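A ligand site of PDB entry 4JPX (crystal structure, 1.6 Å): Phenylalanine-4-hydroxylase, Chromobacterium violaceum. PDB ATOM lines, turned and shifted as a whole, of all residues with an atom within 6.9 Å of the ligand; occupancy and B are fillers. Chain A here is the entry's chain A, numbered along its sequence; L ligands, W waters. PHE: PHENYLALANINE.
The backbone carbonyl oxygen (O) of Pro 261 is in hydrogen-bond range of a nitrogen (N) of the ligand (2.7 Å). The backbone carbonyl oxygen of Thr 259 sits at hydrogen-bond distance from a nitrogen (N) of the ligand. NZ of Lys 170 lies within salt-bridge range of O of the ligand. O of the ligand is in hydrogen-bond range of N of Phe 263, at 3.0 Å.
OG1 of Thr 259 is in hydrogen-bond range of O of Phe 256 (3.2 Å). The backbone carbonyl oxygen (O) of Leu 255 lies within hydrogen-bond range of the side-chain hydroxyl (OG1) of Thr 259, at 2.9 Å. The side-chain amino group (NZ) of Lys 170 is in salt-bridge range of the side-chain carboxylate (OD1) of Asp 262, at 2.7 Å. OD1 of Asp 262 is in hydrogen-bond range of N of Ala 264 (3.0 Å). OH of Tyr 164 lies within hydrogen-bond range of O of Leu 180.
Residues that only touch the ligand: Asp 262, Ala 163, Ala 260, Tyr 164, Leu 183, Leu 180, Tyr 160 and Gly 167. Hydrophobic or aromatic side chains within 4 Å of the ligand: Tyr 160, Ala 163, Tyr 164, Leu 180, Leu 183 and Phe 263. Along chain A the residues within 4 Å of the ligand span positions 160 to 263. The nearest printed residue that does not touch the ligand is Tyr 267 (4.6 Å).
Water W3 lies within hydrogen-bond range of an oxygen (OXT) of the ligand (2.6 Å), the side-chain hydroxyl (OH) of Tyr 267 (2.6 Å) and the backbone carbonyl oxygen (O) of Gly 167 (2.7 Å).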
ATOM      1  N   ASP A 159       6.476  -1.021  24.948  1.00  0.00           N
ATOM      2  CA  ASP A 159       7.212   0.237  24.938  1.00  0.00           C
ATOM      3  C   ASP A 159       6.304   1.430  24.640  1.00  0.00           C
ATOM      4  O   ASP A 159       6.475   2.499  25.203  1.00  0.00           O
ATOM      5  CB  ASP A 159       8.352   0.203  23.916  1.00  0.00           C
ATOM      6  CG  ASP A 159       9.565  -0.537  24.418  1.00  0.00           C
ATOM      7  OD1 ASP A 159       9.645  -0.855  25.618  1.00  0.00           O
ATOM      8  OD2 ASP A 159      10.454  -0.795  23.577  1.00  0.00           O
ATOM      9  N   TYR A 160       5.343   1.234  23.738  1.00  0.00           N
ATOM     10  CA  TYR A 160       4.363   2.281  23.450  1.00  0.00           C
ATOM     11  C   TYR A 160       3.595   2.666  24.717  1.00  0.00           C
ATOM     12  O   TYR A 160       3.437   3.850  25.033  1.00  0.00           O
ATOM     13  CB  TYR A 160       3.438   1.827  22.324  1.00  0.00           C
ATOM     14  CG  TYR A 160       2.258   2.750  22.071  1.00  0.00           C
ATOM     15  CD1 TYR A 160       2.469   4.069  21.656  1.00  0.00           C
ATOM     16  CD2 TYR A 160       0.962   2.303  22.220  1.00  0.00           C
ATOM     17  CE1 TYR A 160       1.396   4.919  21.422  1.00  0.00           C
ATOM     18  CE2 TYR A 160      -0.112   3.152  21.986  1.00  0.00           C
ATOM     19  CZ  TYR A 160       0.108   4.449  21.570  1.00  0.00           C
ATOM     20  OH  TYR A 160      -0.963   5.290  21.331  1.00  0.00           O
ATOM     21  N   LEU A 161       3.137   1.671  25.459  1.00  0.00           N
ATOM     22  CA  LEU A 161       2.387   1.958  26.690  1.00  0.00           C
ATOM     23  C   LEU A 161       3.242   2.636  27.749  1.00  0.00           C
ATOM     24  O   LEU A 161       2.789   3.557  28.414  1.00  0.00           O
ATOM     25  CB  LEU A 161       1.756   0.690  27.264  1.00  0.00           C
ATOM     26  CG  LEU A 161       0.503   0.147  26.585  1.00  0.00           C
ATOM     27  CD1 LEU A 161      -0.088  -0.936  27.476  1.00  0.00           C
ATOM     28  CD2 LEU A 161      -0.532   1.226  26.320  1.00  0.00           C
ATOM     29  N   GLU A 162       4.482   2.187  27.910  1.00  0.00           N
ATOM     30  CA  GLU A 162       5.394   2.837  28.842  1.00  0.00           C
ATOM     31  C   GLU A 162       5.625   4.304  28.427  1.00  0.00           C
ATOM     32  O   GLU A 162       5.589   5.201  29.270  1.00  0.00           O
ATOM     33  CB  GLU A 162       6.721   2.077  28.920  1.00  0.00           C
ATOM     34  CG  GLU A 162       7.674   2.631  29.959  1.00  0.00           C
ATOM     35  CD  GLU A 162       9.063   2.029  29.906  1.00  0.00           C
ATOM     36  OE1 GLU A 162       9.260   0.984  29.252  1.00  0.00           O
ATOM     37  OE2 GLU A 162       9.970   2.603  30.526  1.00  0.00           O
ATOM     38  N   ALA A 163       5.842   4.557  27.139  1.00  0.00           N
ATOM     39  CA  ALA A 163       6.053   5.917  26.653  1.00  0.00           C
ATOM     40  C   ALA A 163       4.813   6.774  26.872  1.00  0.00           C
ATOM     41  O   ALA A 163       4.904   7.942  27.256  1.00  0.00           O
ATOM     42  CB  ALA A 163       6.429   5.880  25.182  1.00  0.00           C
ATOM     43  N   TYR A 164       3.648   6.177  26.656  1.00  0.00           N
ATOM     44  CA  TYR A 164       2.388   6.874  26.892  1.00  0.00           C
ATOM     45  C   TYR A 164       2.305   7.279  28.366  1.00  0.00           C
ATOM     46  O   TYR A 164       2.011   8.442  28.691  1.00  0.00           O
ATOM     47  CB  TYR A 164       1.204   5.994  26.498  1.00  0.00           C
ATOM     48  CG  TYR A 164      -0.140   6.613  26.803  1.00  0.00           C
ATOM     49  CD1 TYR A 164      -0.776   7.431  25.881  1.00  0.00           C
ATOM     50  CD2 TYR A 164      -0.773   6.373  28.028  1.00  0.00           C
ATOM     51  CE1 TYR A 164      -1.989   8.022  26.172  1.00  0.00           C
ATOM     52  CE2 TYR A 164      -1.988   6.950  28.320  1.00  0.00           C
ATOM     53  CZ  TYR A 164      -2.600   7.764  27.396  1.00  0.00           C
ATOM     54  OH  TYR A 164      -3.811   8.347  27.681  1.00  0.00           O
ATOM     55  N   GLY A 165       2.589   6.337  29.263  1.00  0.00           N
ATOM     56  CA  GLY A 165       2.597   6.611  30.690  1.00  0.00           C
ATOM     57  C   GLY A 165       3.498   7.778  31.037  1.00  0.00           C
ATOM     58  O   GLY A 165       3.086   8.715  31.715  1.00  0.00           O
ATOM     59  N   LYS A 166       4.730   7.735  30.540  1.00  0.00           N
ATOM     60  CA  LYS A 166       5.704   8.809  30.801  1.00  0.00           C
ATOM     61  C   LYS A 166       5.241  10.166  30.273  1.00  0.00           C
ATOM     62  O   LYS A 166       5.569  11.203  30.839  1.00  0.00           O
ATOM     63  CB  LYS A 166       7.066   8.441  30.222  1.00  0.00           C
ATOM     64  CG  LYS A 166       7.693   7.273  30.955  1.00  0.00           C
ATOM     65  CD  LYS A 166       9.006   6.840  30.325  1.00  0.00           C
ATOM     66  CE  LYS A 166       9.681   5.784  31.201  1.00  0.00           C
ATOM     67  NZ  LYS A 166      10.935   5.275  30.596  1.00  0.00           N
ATOM     68  N   GLY A 167       4.448  10.159  29.205  1.00  0.00           N
ATOM     69  CA  GLY A 167       3.904  11.369  28.602  1.00  0.00           C
ATOM     70  C   GLY A 167       2.830  12.065  29.423  1.00  0.00           C
ATOM     71  O   GLY A 167       2.462  13.201  29.123  1.00  0.00           O
ATOM     72  N   GLY A 168       2.324  11.404  30.470  1.00  0.00           N
ATOM     73  CA  GLY A 168       1.244  11.971  31.271  1.00  0.00           C
ATOM     74  C   GLY A 168       1.627  13.222  32.035  1.00  0.00           C
ATOM     75  O   GLY A 168       0.811  14.131  32.198  1.00  0.00           O
ATOM     76  N   LYS A 170       3.811  15.679  31.166  1.00  0.00           N
ATOM     77  CA  LYS A 170       3.750  16.808  30.249  1.00  0.00           C
ATOM     78  C   LYS A 170       2.316  17.203  29.928  1.00  0.00           C
ATOM     79  O   LYS A 170       1.977  18.388  29.932  1.00  0.00           O
ATOM     80  CB  LYS A 170       4.506  16.467  28.954  1.00  0.00           C
ATOM     81  CG  LYS A 170       4.632  17.620  27.958  1.00  0.00           C
ATOM     82  CD  LYS A 170       5.272  17.182  26.660  1.00  0.00           C
ATOM     83  CE  LYS A 170       6.761  16.938  26.820  1.00  0.00           C
ATOM     84  NZ  LYS A 170       7.382  16.624  25.503  1.00  0.00           N
ATOM     85  N   ALA A 171       1.474  16.223  29.664  1.00  0.00           N
ATOM     86  CA  ALA A 171       0.084  16.487  29.296  1.00  0.00           C
ATOM     87  C   ALA A 171      -0.652  17.192  30.442  1.00  0.00           C
ATOM     88  O   ALA A 171      -1.359  18.185  30.232  1.00  0.00           O
ATOM     89  CB  ALA A 171      -0.633  15.217  28.886  1.00  0.00           C
ATOM     90  N   LEU A 180      -4.332  13.335  25.132  1.00  0.00           N
ATOM     91  CA  LEU A 180      -3.736  12.007  25.314  1.00  0.00           C
ATOM     92  C   LEU A 180      -4.807  10.938  25.487  1.00  0.00           C
ATOM     93  O   LEU A 180      -4.664   9.835  24.974  1.00  0.00           O
ATOM     94  CB  LEU A 180      -2.785  11.937  26.512  1.00  0.00           C
ATOM     95  CG  LEU A 180      -1.331  12.337  26.320  1.00  0.00           C
ATOM     96  CD1 LEU A 180      -0.534  11.963  27.552  1.00  0.00           C
ATOM     97  CD2 LEU A 180      -0.739  11.666  25.089  1.00  0.00           C
ATOM     98  N   LEU A 183      -5.944   9.817  22.145  1.00  0.00           N
ATOM     99  CA  LEU A 183      -4.944   8.932  21.527  1.00  0.00           C
ATOM    100  C   LEU A 183      -5.049   7.524  22.102  1.00  0.00           C
ATOM    101  O   LEU A 183      -5.046   6.564  21.362  1.00  0.00           O
ATOM    102  CB  LEU A 183      -3.532   9.483  21.748  1.00  0.00           C
ATOM    103  CG  LEU A 183      -2.394   8.623  21.220  1.00  0.00           C
ATOM    104  CD1 LEU A 183      -2.500   8.404  19.715  1.00  0.00           C
ATOM    105  CD2 LEU A 183      -1.072   9.272  21.582  1.00  0.00           C
ATOM    106  N   LEU A 229      -1.624  11.271  13.944  1.00  0.00           N
ATOM    107  CA  LEU A 229      -1.506  11.671  15.352  1.00  0.00           C
ATOM    108  C   LEU A 229      -2.327  12.917  15.682  1.00  0.00           C
ATOM    109  O   LEU A 229      -3.105  12.919  16.632  1.00  0.00           O
ATOM    110  CB  LEU A 229      -0.044  11.897  15.731  1.00  0.00           C
ATOM    111  CG  LEU A 229       0.196  12.470  17.128  1.00  0.00           C
ATOM    112  CD1 LEU A 229      -0.382  11.572  18.222  1.00  0.00           C
ATOM    113  CD2 LEU A 229       1.670  12.747  17.377  1.00  0.00           C
ATOM    114  N   MET A 233      -5.743  13.222  18.121  1.00  0.00           N
ATOM    115  CA  MET A 233      -5.756  13.995  19.360  1.00  0.00           C
ATOM    116  C   MET A 233      -6.754  15.154  19.292  1.00  0.00           C
ATOM    117  O   MET A 233      -7.075  15.753  20.316  1.00  0.00           O
ATOM    118  CB  MET A 233      -4.348  14.467  19.751  1.00  0.00           C
ATOM    119  CG  MET A 233      -3.463  13.310  20.178  1.00  0.00           C
ATOM    120  SD  MET A 233      -2.049  13.769  21.202  1.00  0.00           S
ATOM    121  CE  MET A 233      -1.081  14.777  20.083  1.00  0.00           C
ATOM    122  N   LEU A 255       3.178   2.983  15.029  1.00  0.00           N
ATOM    123  CA  LEU A 255       2.519   3.652  16.133  1.00  0.00           C
ATOM    124  C   LEU A 255       3.522   4.212  17.150  1.00  0.00           C
ATOM    125  O   LEU A 255       3.391   5.360  17.592  1.00  0.00           O
ATOM    126  CB  LEU A 255       1.535   2.694  16.789  1.00  0.00           C
ATOM    127  CG  LEU A 255       0.796   3.138  18.039  1.00  0.00           C
ATOM    128  CD1 LEU A 255      -0.022   4.396  17.742  1.00  0.00           C
ATOM    129  CD2 LEU A 255      -0.092   1.993  18.503  1.00  0.00           C
ATOM    130  N   PHE A 256       4.542   3.418  17.510  1.00  0.00           N
ATOM    131  CA  PHE A 256       5.572   3.899  18.439  1.00  0.00           C
ATOM    132  C   PHE A 256       6.335   5.095  17.841  1.00  0.00           C
ATOM    133  O   PHE A 256       6.533   6.120  18.490  1.00  0.00           O
ATOM    134  CB  PHE A 256       6.572   2.787  18.819  1.00  0.00           C
ATOM    135  CG  PHE A 256       7.616   3.246  19.799  1.00  0.00           C
ATOM    136  CD1 PHE A 256       7.380   3.163  21.160  1.00  0.00           C
ATOM    137  CD2 PHE A 256       8.798   3.808  19.352  1.00  0.00           C
ATOM    138  CE1 PHE A 256       8.330   3.604  22.058  1.00  0.00           C
ATOM    139  CE2 PHE A 256       9.755   4.256  20.261  1.00  0.00           C
ATOM    140  CZ  PHE A 256       9.518   4.151  21.616  1.00  0.00           C
ATOM    141  N   ALA A 258       5.457   7.163  15.397  1.00  0.00           N
ATOM    142  CA  ALA A 258       4.585   8.316  15.148  1.00  0.00           C
ATOM    143  C   ALA A 258       4.300   9.112  16.420  1.00  0.00           C
ATOM    144  O   ALA A 258       3.983  10.299  16.345  1.00  0.00           O
ATOM    145  CB  ALA A 258       3.290   7.874  14.506  1.00  0.00           C
ATOM    146  N   THR A 259       4.403   8.458  17.561  1.00  0.00           N
ATOM    147  CA  THR A 259       4.124   9.103  18.847  1.00  0.00           C
ATOM    148  C   THR A 259       5.388   9.469  19.644  1.00  0.00           C
ATOM    149  O   THR A 259       5.285   9.908  20.777  1.00  0.00           O
ATOM    150  CB  THR A 259       3.180   8.218  19.712  1.00  0.00           C
ATOM    151  OG1 THR A 259       3.787   6.941  19.967  1.00  0.00           O
ATOM    152  CG2 THR A 259       1.833   8.024  18.977  1.00  0.00           C
ATOM    153  N   ALA A 260       6.569   9.330  19.033  1.00  0.00           N
ATOM    154  CA  ALA A 260       7.847   9.647  19.713  1.00  0.00           C
ATOM    155  C   ALA A 260       8.263  11.145  19.772  1.00  0.00           C
ATOM    156  O   ALA A 260       8.983  11.538  20.694  1.00  0.00           O
ATOM    157  CB  ALA A 260       8.967   8.808  19.100  1.00  0.00           C
ATOM    158  N   PRO A 261       7.834  11.964  18.794  1.00  0.00           N
ATOM    159  CA  PRO A 261       8.168  13.397  18.857  1.00  0.00           C
ATOM    160  C   PRO A 261       7.558  14.162  20.041  1.00  0.00           C
ATOM    161  O   PRO A 261       6.668  13.663  20.723  1.00  0.00           O
ATOM    162  CB  PRO A 261       7.594  13.940  17.540  1.00  0.00           C
ATOM    163  CG  PRO A 261       7.562  12.764  16.628  1.00  0.00           C
ATOM    164  CD  PRO A 261       7.212  11.606  17.507  1.00  0.00           C
ATOM    165  N   ASP A 262       8.052  15.381  20.260  1.00  0.00           N
ATOM    166  CA  ASP A 262       7.607  16.280  21.331  1.00  0.00           C
ATOM    167  C   ASP A 262       6.155  16.724  21.093  1.00  0.00           C
ATOM    168  O   ASP A 262       5.842  17.374  20.095  1.00  0.00           O
ATOM    169  CB  ASP A 262       8.543  17.496  21.406  1.00  0.00           C
ATOM    170  CG  ASP A 262       8.125  18.533  22.443  1.00  0.00           C
ATOM    171  OD1 ASP A 262       7.331  18.206  23.361  1.00  0.00           O
ATOM    172  OD2 ASP A 262       8.607  19.692  22.345  1.00  0.00           O
ATOM    173  N   PHE A 263       5.270  16.384  22.027  1.00  0.00           N
ATOM    174  CA  PHE A 263       3.859  16.725  21.874  1.00  0.00           C
ATOM    175  C   PHE A 263       3.524  18.149  22.313  1.00  0.00           C
ATOM    176  O   PHE A 263       2.422  18.621  22.039  1.00  0.00           O
ATOM    177  CB  PHE A 263       2.978  15.755  22.670  1.00  0.00           C
ATOM    178  CG  PHE A 263       2.754  14.406  22.031  1.00  0.00           C
ATOM    179  CD1 PHE A 263       3.579  13.907  21.023  1.00  0.00           C
ATOM    180  CD2 PHE A 263       1.711  13.600  22.481  1.00  0.00           C
ATOM    181  CE1 PHE A 263       3.352  12.647  20.469  1.00  0.00           C
ATOM    182  CE2 PHE A 263       1.480  12.355  21.939  1.00  0.00           C
ATOM    183  CZ  PHE A 263       2.311  11.863  20.941  1.00  0.00           C
ATOM    184  N   ALA A 264       4.447  18.837  22.993  1.00  0.00           N
ATOM    185  CA  ALA A 264       4.117  20.138  23.614  1.00  0.00           C
ATOM    186  C   ALA A 264       3.587  21.151  22.596  1.00  0.00           C
ATOM    187  O   ALA A 264       2.516  21.745  22.804  1.00  0.00           O
ATOM    188  CB  ALA A 264       5.323  20.706  24.361  1.00  0.00           C
ATOM    189  N   TYR A 267       0.044  20.003  21.475  1.00  0.00           N
ATOM    190  CA  TYR A 267      -0.978  20.318  22.478  1.00  0.00           C
ATOM    191  C   TYR A 267      -1.449  21.765  22.391  1.00  0.00           C
ATOM    192  O   TYR A 267      -2.658  22.022  22.393  1.00  0.00           O
ATOM    193  CB  TYR A 267      -0.456  20.059  23.893  1.00  0.00           C
ATOM    194  CG  TYR A 267      -0.203  18.607  24.258  1.00  0.00           C
ATOM    195  CD1 TYR A 267      -0.994  17.568  23.770  1.00  0.00           C
ATOM    196  CD2 TYR A 267       0.812  18.278  25.143  1.00  0.00           C
ATOM    197  CE1 TYR A 267      -0.754  16.246  24.128  1.00  0.00           C
ATOM    198  CE2 TYR A 267       1.056  16.971  25.517  1.00  0.00           C
ATOM    199  CZ  TYR A 267       0.276  15.958  25.015  1.00  0.00           C
ATOM    200  OH  TYR A 267       0.542  14.663  25.416  1.00  0.00           O
HETATM  201  N   PHE L   1       5.962  11.914  22.685  1.00  0.00           N
HETATM  202  CA  PHE L   1       5.070  12.298  23.784  1.00  0.00           C
HETATM  203  C   PHE L   1       5.542  13.575  24.480  1.00  0.00           C
HETATM  204  O   PHE L   1       6.351  14.329  23.940  1.00  0.00           O
HETATM  205  CB  PHE L   1       4.934  11.154  24.798  1.00  0.00           C
HETATM  206  CG  PHE L   1       4.049  10.045  24.314  1.00  0.00           C
HETATM  207  CD1 PHE L   1       2.661  10.194  24.320  1.00  0.00           C
HETATM  208  CD2 PHE L   1       4.589   8.873  23.843  1.00  0.00           C
HETATM  209  CE1 PHE L   1       1.843   9.174  23.862  1.00  0.00           C
HETATM  210  CE2 PHE L   1       3.778   7.839  23.391  1.00  0.00           C
HETATM  211  CZ  PHE L   1       2.403   7.993  23.395  1.00  0.00           C
HETATM  212  OXT PHE L   1       5.110  13.907  25.574  1.00  0.00           O
HETATM  213  O   HOH W   1       8.271  10.224  23.884  1.00  0.00           O
HETATM  214  O   HOH W   2       6.824  13.801  27.699  1.00  0.00           O
HETATM  215  O   HOH W   3       2.793  14.236  26.611  1.00  0.00           O
HETATM  216  O   HOH W   4       9.565  14.346  23.889  1.00  0.00           O
